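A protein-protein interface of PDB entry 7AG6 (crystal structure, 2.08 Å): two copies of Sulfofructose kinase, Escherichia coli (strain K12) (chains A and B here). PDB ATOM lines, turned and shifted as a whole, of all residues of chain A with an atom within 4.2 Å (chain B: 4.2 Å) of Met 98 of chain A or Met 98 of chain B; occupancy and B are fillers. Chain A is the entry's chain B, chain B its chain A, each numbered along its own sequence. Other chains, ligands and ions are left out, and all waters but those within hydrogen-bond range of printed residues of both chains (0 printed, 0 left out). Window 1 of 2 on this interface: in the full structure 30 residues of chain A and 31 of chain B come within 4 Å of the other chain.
Printed residues of chain A that touch a printed residue of chain B: Tyr 16, Pro 22, Met 98, Ile 106 and Ile 108. Hydrophobic or aromatic side chains of chain A that line the printed part of chain B: Tyr 16, Pro 22, Met 98, Ile 106 and Ile 108. Along chain A the printed residues that touch a printed residue of chain B span positions 16 to 108. Among the printed residues, no Asp or Glu carboxylate lies within 4 Å of a Lys or Arg side-chain nitrogen of the other chain.
CB of Ala 96 of chain B touches CE1 of Tyr 16 of chain A, 3.6 Å away. CB of Tyr 16 of chain A touches CG2 of Ile 108 of chain B, at 3.8 Å. CG2 of Ile 106 of chain B touches CB of Pro 22 of chain A, 3.9 Å away. Met 98 of chain A touches Met 98 of chain B. Met 98 of chain A touches Ile 108 of chain B (SD to CG1, 3.8 Å). Ile 106 of chain A touches Pro 22 of chain B (CG2 to CB, 3.7 Å). Ile 108 of chain A touches Tyr 16 of chain B. Ile 108 of chain A touches Pro 22 of chain B.
The backbone carbonyl oxygen (O) of Pro 22 of chain A lies close to the backbone carbonyl oxygen (O) of Pro 22 of chain B, at 3.3 Å.
Tyr 16 of chain A touches Ile 108 of chain B, and with the chains exchanged Ile 108 of chain A touches Tyr 16 of chain B. Pro 22 of chain B touches its own counterpart, Pro 22 of chain A. Met 98 of chain A touches its own counterpart, Met 98 of chain B. Met 98 of chain A touches Ile 108 of chain B, but with the chains exchanged Ile 108 of chain A does not touch Met 98 of chain B (4.02 Å).
O of Ile 106 of chain B lies within hydrogen-bond range of N of Met 98 of chain B, 2.8 Å away. N of Met 98 of chain A is in hydrogen-bond range of O of Ile 106 of chain A (2.8 Å). O of Tyr 16 of chain A is in hydrogen-bond range of N of Val 99 of chain A (2.8 Å). The backbone carbonyl oxygen of Tyr 16 of chain B lies within hydrogen-bond range of the backbone NH of Val 99 of chain B, 2.9 Å away. The backbone carbonyl oxygen of Ile 97 of chain A lies within hydrogen-bond range of the backbone NH of Tyr 16 of chain A (2.7 Å). The backbone NH (N) of Ile 108 of chain B is in hydrogen-bond range of the backbone carbonyl oxygen (O) of Ala 96 of chain B (2.8 Å).
Met 98 of chain A touches two residues of chain B. Of the printed residues of chain A, Met 98 of chain B touches Met 98 (3.4 Å). Printed residues of chain B within 4 Å of Pro 22 of chain A: Pro 22 and Ile 106. Printed residues of chain A within 4 Å of Ile 106 of chain B: Pro 22 (3.9 Å). Of the printed residues of chain B, Ile 106 of chain A touches Pro 22. Printed residues of chain A within 4 Å of Ala 96 of chain B: Tyr 16 (3.6 Å). Of the printed residues of chain A, Ile 108 of chain B touches Tyr 16 (3.8 Å) and Met 98 (3.8 Å). Glu 104 of chain A touches none of the printed residues of chain B. The nearest printed residue of chain B that does not touch Met 98 of chain A is Ile 106 of chain B (5.3 Å).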
ATOM      1  N   TYR A  16      -2.009 -17.771  -3.200  1.00  0.00           N
ATOM      2  CA  TYR A  16      -2.352 -19.088  -2.631  1.00  0.00           C
ATOM      3  C   TYR A  16      -1.231 -19.479  -1.671  1.00  0.00           C
ATOM      4  O   TYR A  16      -0.065 -19.560  -2.102  1.00  0.00           O
ATOM      5  CB  TYR A  16      -2.542 -20.080  -3.783  1.00  0.00           C
ATOM      6  CG  TYR A  16      -3.667 -19.734  -4.725  1.00  0.00           C
ATOM      7  CD1 TYR A  16      -3.466 -18.830  -5.757  1.00  0.00           C
ATOM      8  CD2 TYR A  16      -4.915 -20.317  -4.612  1.00  0.00           C
ATOM      9  CE1 TYR A  16      -4.483 -18.489  -6.637  1.00  0.00           C
ATOM     10  CE2 TYR A  16      -5.939 -20.003  -5.491  1.00  0.00           C
ATOM     11  CZ  TYR A  16      -5.718 -19.090  -6.512  1.00  0.00           C
ATOM     12  OH  TYR A  16      -6.695 -18.729  -7.379  1.00  0.00           O
ATOM     13  N   LEU A  21       5.858 -25.563  -2.374  1.00  0.00           N
ATOM     14  CA  LEU A  21       5.783 -25.153  -3.787  1.00  0.00           C
ATOM     15  C   LEU A  21       5.581 -26.425  -4.599  1.00  0.00           C
ATOM     16  O   LEU A  21       6.279 -27.409  -4.407  1.00  0.00           O
ATOM     17  CB  LEU A  21       7.023 -24.356  -4.186  1.00  0.00           C
ATOM     18  CG  LEU A  21       7.113 -22.975  -3.522  1.00  0.00           C
ATOM     19  CD1 LEU A  21       8.349 -22.235  -4.006  1.00  0.00           C
ATOM     20  CD2 LEU A  21       5.861 -22.123  -3.767  1.00  0.00           C
ATOM     21  N   PRO A  22       4.552 -26.482  -5.466  1.00  0.00           N
ATOM     22  CA  PRO A  22       4.384 -27.626  -6.352  1.00  0.00           C
ATOM     23  C   PRO A  22       5.642 -27.855  -7.211  1.00  0.00           C
ATOM     24  O   PRO A  22       6.016 -26.982  -7.969  1.00  0.00           O
ATOM     25  CB  PRO A  22       3.140 -27.244  -7.169  1.00  0.00           C
ATOM     26  CG  PRO A  22       3.068 -25.748  -7.067  1.00  0.00           C
ATOM     27  CD  PRO A  22       3.522 -25.453  -5.657  1.00  0.00           C
ATOM     28  N   ILE A  97      -0.214 -16.494  -7.620  1.00  0.00           N
ATOM     29  CA  ILE A  97       1.036 -16.591  -6.825  1.00  0.00           C
ATOM     30  C   ILE A  97       0.874 -17.733  -5.815  1.00  0.00           C
ATOM     31  O   ILE A  97      -0.176 -17.834  -5.180  1.00  0.00           O
ATOM     32  CB  ILE A  97       1.365 -15.233  -6.161  1.00  0.00           C
ATOM     33  CG1 ILE A  97       1.435 -14.096  -7.182  1.00  0.00           C
ATOM     34  CG2 ILE A  97       2.660 -15.367  -5.361  1.00  0.00           C
ATOM     35  CD1 ILE A  97       1.785 -12.720  -6.601  1.00  0.00           C
ATOM     36  N   MET A  98       1.894 -18.554  -5.670  1.00  0.00           N
ATOM     37  CA  MET A  98       1.923 -19.621  -4.661  1.00  0.00           C
ATOM     38  C   MET A  98       3.059 -19.302  -3.698  1.00  0.00           C
ATOM     39  O   MET A  98       4.224 -19.172  -4.165  1.00  0.00           O
ATOM     40  CB  MET A  98       2.205 -20.977  -5.311  1.00  0.00           C
ATOM     41  CG  MET A  98       1.011 -21.653  -5.875  1.00  0.00           C
ATOM     42  SD  MET A  98       1.505 -22.383  -7.431  1.00  0.00           S
ATOM     43  CE  MET A  98       1.091 -20.971  -8.464  1.00  0.00           C
ATOM     44  N   VAL A  99       2.725 -19.224  -2.420  1.00  0.00           N
ATOM     45  CA  VAL A  99       3.658 -18.912  -1.306  1.00  0.00           C
ATOM     46  C   VAL A  99       3.688 -20.126  -0.377  1.00  0.00           C
ATOM     47  O   VAL A  99       2.609 -20.552   0.048  1.00  0.00           O
ATOM     48  CB  VAL A  99       3.193 -17.644  -0.569  1.00  0.00           C
ATOM     49  CG1 VAL A  99       4.143 -17.291   0.571  1.00  0.00           C
ATOM     50  CG2 VAL A  99       3.018 -16.475  -1.539  1.00  0.00           C
ATOM     51  N   GLU A 104       8.689 -18.384   0.378  1.00  0.00           N
ATOM     52  CA  GLU A 104       9.170 -18.481  -1.027  1.00  0.00           C
ATOM     53  C   GLU A 104       7.951 -18.544  -1.958  1.00  0.00           C
ATOM     54  O   GLU A 104       6.906 -19.081  -1.543  1.00  0.00           O
ATOM     55  CB  GLU A 104      10.078 -19.695  -1.212  1.00  0.00           C
ATOM     56  CG  GLU A 104      11.403 -19.598  -0.459  1.00  0.00           C
ATOM     57  CD  GLU A 104      12.231 -18.323  -0.633  1.00  0.00           C
ATOM     58  OE1 GLU A 104      12.743 -18.085  -1.746  1.00  0.00           O
ATOM     59  OE2 GLU A 104      12.376 -17.564   0.353  1.00  0.00           O
ATOM     60  N   ARG A 105       8.064 -17.999  -3.173  1.00  0.00           N
ATOM     61  CA  ARG A 105       6.880 -17.798  -4.053  1.00  0.00           C
ATOM     62  C   ARG A 105       7.199 -18.142  -5.514  1.00  0.00           C
ATOM     63  O   ARG A 105       8.355 -17.974  -5.965  1.00  0.00           O
ATOM     64  CB  ARG A 105       6.307 -16.382  -3.887  1.00  0.00           C
ATOM     65  CG  ARG A 105       6.906 -15.306  -4.785  1.00  0.00           C
ATOM     66  CD  ARG A 105       8.266 -14.861  -4.311  1.00  0.00           C
ATOM     67  NE  ARG A 105       8.806 -13.773  -5.115  1.00  0.00           N
ATOM     68  CZ  ARG A 105       9.471 -13.907  -6.261  1.00  0.00           C
ATOM     69  NH1 ARG A 105       9.923 -12.821  -6.857  1.00  0.00           N
ATOM     70  NH2 ARG A 105       9.640 -15.090  -6.835  1.00  0.00           N
ATOM     71  N   ILE A 106       6.190 -18.692  -6.179  1.00  0.00           N
ATOM     72  CA  ILE A 106       6.094 -18.837  -7.652  1.00  0.00           C
ATOM     73  C   ILE A 106       5.020 -17.852  -8.096  1.00  0.00           C
ATOM     74  O   ILE A 106       3.926 -17.858  -7.499  1.00  0.00           O
ATOM     75  CB  ILE A 106       5.758 -20.281  -8.049  1.00  0.00           C
ATOM     76  CG1 ILE A 106       6.940 -21.226  -7.813  1.00  0.00           C
ATOM     77  CG2 ILE A 106       5.273 -20.344  -9.482  1.00  0.00           C
ATOM     78  CD1 ILE A 106       6.565 -22.682  -7.840  1.00  0.00           C
ATOM     79  N   ILE A 108       2.969 -16.484 -11.482  1.00  0.00           N
ATOM     80  CA  ILE A 108       2.558 -16.643 -12.901  1.00  0.00           C
ATOM     81  C   ILE A 108       1.822 -15.364 -13.268  1.00  0.00           C
ATOM     82  O   ILE A 108       0.715 -15.175 -12.737  1.00  0.00           O
ATOM     83  CB  ILE A 108       1.644 -17.870 -13.111  1.00  0.00           C
ATOM     84  CG1 ILE A 108       2.120 -19.113 -12.361  1.00  0.00           C
ATOM     85  CG2 ILE A 108       1.466 -18.114 -14.595  1.00  0.00           C
ATOM     86  CD1 ILE A 108       3.461 -19.613 -12.813  1.00  0.00           C
ATOM     87  N   TYR B  16      -3.937 -20.796 -16.481  1.00  0.00           N
ATOM     88  CA  TYR B  16      -2.724 -20.163 -17.017  1.00  0.00           C
ATOM     89  C   TYR B  16      -2.018 -21.202 -17.893  1.00  0.00           C
ATOM     90  O   TYR B  16      -1.609 -22.262 -17.382  1.00  0.00           O
ATOM     91  CB  TYR B  16      -1.863 -19.676 -15.846  1.00  0.00           C
ATOM     92  CG  TYR B  16      -2.528 -18.633 -14.967  1.00  0.00           C
ATOM     93  CD1 TYR B  16      -3.419 -19.012 -13.978  1.00  0.00           C
ATOM     94  CD2 TYR B  16      -2.279 -17.275 -15.113  1.00  0.00           C
ATOM     95  CE1 TYR B  16      -4.050 -18.089 -13.171  1.00  0.00           C
ATOM     96  CE2 TYR B  16      -2.896 -16.327 -14.301  1.00  0.00           C
ATOM     97  CZ  TYR B  16      -3.773 -16.743 -13.311  1.00  0.00           C
ATOM     98  OH  TYR B  16      -4.429 -15.894 -12.476  1.00  0.00           O
ATOM     99  N   LEU B  21       5.595 -26.402 -16.674  1.00  0.00           N
ATOM    100  CA  LEU B  21       5.064 -26.311 -15.299  1.00  0.00           C
ATOM    101  C   LEU B  21       6.126 -25.655 -14.426  1.00  0.00           C
ATOM    102  O   LEU B  21       7.282 -26.029 -14.493  1.00  0.00           O
ATOM    103  CB  LEU B  21       4.652 -27.699 -14.815  1.00  0.00           C
ATOM    104  CG  LEU B  21       3.433 -28.271 -15.529  1.00  0.00           C
ATOM    105  CD1 LEU B  21       3.115 -29.660 -15.011  1.00  0.00           C
ATOM    106  CD2 LEU B  21       2.213 -27.369 -15.382  1.00  0.00           C
ATOM    107  N   PRO B  22       5.788 -24.593 -13.676  1.00  0.00           N
ATOM    108  CA  PRO B  22       6.755 -23.961 -12.777  1.00  0.00           C
ATOM    109  C   PRO B  22       7.170 -24.917 -11.643  1.00  0.00           C
ATOM    110  O   PRO B  22       6.384 -25.132 -10.729  1.00  0.00           O
ATOM    111  CB  PRO B  22       5.997 -22.734 -12.262  1.00  0.00           C
ATOM    112  CG  PRO B  22       4.540 -23.075 -12.453  1.00  0.00           C
ATOM    113  CD  PRO B  22       4.487 -23.913 -13.703  1.00  0.00           C
ATOM    114  N   ALA B  96      -6.416 -21.888  -9.090  1.00  0.00           N
ATOM    115  CA  ALA B  96      -5.422 -21.475 -10.101  1.00  0.00           C
ATOM    116  C   ALA B  96      -4.888 -22.750 -10.755  1.00  0.00           C
ATOM    117  O   ALA B  96      -4.472 -23.670 -10.036  1.00  0.00           O
ATOM    118  CB  ALA B  96      -4.328 -20.643  -9.475  1.00  0.00           C
ATOM    119  N   ILE B  97      -4.881 -22.789 -12.077  1.00  0.00           N
ATOM    120  CA  ILE B  97      -4.435 -24.003 -12.817  1.00  0.00           C
ATOM    121  C   ILE B  97      -3.358 -23.593 -13.821  1.00  0.00           C
ATOM    122  O   ILE B  97      -3.505 -22.569 -14.494  1.00  0.00           O
ATOM    123  CB  ILE B  97      -5.632 -24.707 -13.473  1.00  0.00           C
ATOM    124  CG1 ILE B  97      -6.725 -25.048 -12.456  1.00  0.00           C
ATOM    125  CG2 ILE B  97      -5.157 -25.941 -14.221  1.00  0.00           C
ATOM    126  CD1 ILE B  97      -7.941 -25.750 -13.022  1.00  0.00           C
ATOM    127  N   MET B  98      -2.265 -24.331 -13.832  1.00  0.00           N
ATOM    128  CA  MET B  98      -1.170 -24.119 -14.807  1.00  0.00           C
ATOM    129  C   MET B  98      -1.154 -25.330 -15.747  1.00  0.00           C
ATOM    130  O   MET B  98      -1.036 -26.458 -15.242  1.00  0.00           O
ATOM    131  CB  MET B  98       0.176 -24.013 -14.106  1.00  0.00           C
ATOM    132  CG  MET B  98       0.418 -22.689 -13.430  1.00  0.00           C
ATOM    133  SD  MET B  98       1.067 -22.949 -11.763  1.00  0.00           S
ATOM    134  CE  MET B  98      -0.491 -22.763 -10.893  1.00  0.00           C
ATOM    135  N   VAL B  99      -1.286 -25.082 -17.048  1.00  0.00           N
ATOM    136  CA  VAL B  99      -1.304 -26.121 -18.102  1.00  0.00           C
ATOM    137  C   VAL B  99      -0.078 -25.893 -19.000  1.00  0.00           C
ATOM    138  O   VAL B  99       0.077 -24.773 -19.491  1.00  0.00           O
ATOM    139  CB  VAL B  99      -2.624 -26.069 -18.890  1.00  0.00           C
ATOM    140  CG1 VAL B  99      -2.674 -27.134 -19.981  1.00  0.00           C
ATOM    141  CG2 VAL B  99      -3.837 -26.203 -17.977  1.00  0.00           C
ATOM    142  N   GLU B 104      -0.490 -31.190 -19.539  1.00  0.00           N
ATOM    143  CA  GLU B 104      -0.319 -31.579 -18.110  1.00  0.00           C
ATOM    144  C   GLU B 104      -0.593 -30.348 -17.233  1.00  0.00           C
ATOM    145  O   GLU B 104      -0.317 -29.233 -17.695  1.00  0.00           O
ATOM    146  CB  GLU B 104       1.084 -32.150 -17.869  1.00  0.00           C
ATOM    147  CG  GLU B 104       1.355 -33.425 -18.666  1.00  0.00           C
ATOM    148  CD  GLU B 104       0.391 -34.566 -18.360  1.00  0.00           C
ATOM    149  OE1 GLU B 104       0.319 -34.995 -17.170  1.00  0.00           O
ATOM    150  OE2 GLU B 104      -0.329 -34.987 -19.291  1.00  0.00           O
ATOM    151  N   ARG B 105      -1.106 -30.538 -16.014  1.00  0.00           N
ATOM    152  CA  ARG B 105      -1.625 -29.410 -15.194  1.00  0.00           C
ATOM    153  C   ARG B 105      -1.204 -29.539 -13.720  1.00  0.00           C
ATOM    154  O   ARG B 105      -1.089 -30.681 -13.156  1.00  0.00           O
ATOM    155  CB  ARG B 105      -3.133 -29.283 -15.404  1.00  0.00           C
ATOM    156  CG  ARG B 105      -4.011 -30.102 -14.475  1.00  0.00           C
ATOM    157  CD  ARG B 105      -4.162 -31.536 -14.907  1.00  0.00           C
ATOM    158  NE  ARG B 105      -5.027 -32.261 -13.964  1.00  0.00           N
ATOM    159  CZ  ARG B 105      -4.614 -32.838 -12.824  1.00  0.00           C
ATOM    160  NH1 ARG B 105      -5.473 -33.475 -12.047  1.00  0.00           N
ATOM    161  NH2 ARG B 105      -3.337 -32.827 -12.484  1.00  0.00           N
ATOM    162  N   ILE B 106      -0.941 -28.383 -13.124  1.00  0.00           N
ATOM    163  CA  ILE B 106      -0.905 -28.172 -11.653  1.00  0.00           C
ATOM    164  C   ILE B 106      -2.180 -27.400 -11.298  1.00  0.00           C
ATOM    165  O   ILE B 106      -2.473 -26.409 -11.959  1.00  0.00           O
ATOM    166  CB  ILE B 106       0.358 -27.426 -11.209  1.00  0.00           C
ATOM    167  CG1 ILE B 106       1.627 -28.254 -11.439  1.00  0.00           C
ATOM    168  CG2 ILE B 106       0.225 -27.004  -9.760  1.00  0.00           C
ATOM    169  CD1 ILE B 106       2.913 -27.515 -11.144  1.00  0.00           C
ATOM    170  N   ILE B 108      -4.101 -25.638  -8.026  1.00  0.00           N
ATOM    171  CA  ILE B 108      -4.113 -25.142  -6.631  1.00  0.00           C
ATOM    172  C   ILE B 108      -5.560 -24.771  -6.342  1.00  0.00           C
ATOM    173  O   ILE B 108      -6.033 -23.753  -6.925  1.00  0.00           O
ATOM    174  CB  ILE B 108      -3.206 -23.921  -6.432  1.00  0.00           C
ATOM    175  CG1 ILE B 108      -1.850 -24.081  -7.128  1.00  0.00           C
ATOM    176  CG2 ILE B 108      -3.094 -23.634  -4.940  1.00  0.00           C
ATOM    177  CD1 ILE B 108      -1.009 -25.183  -6.558  1.00  0.00           C
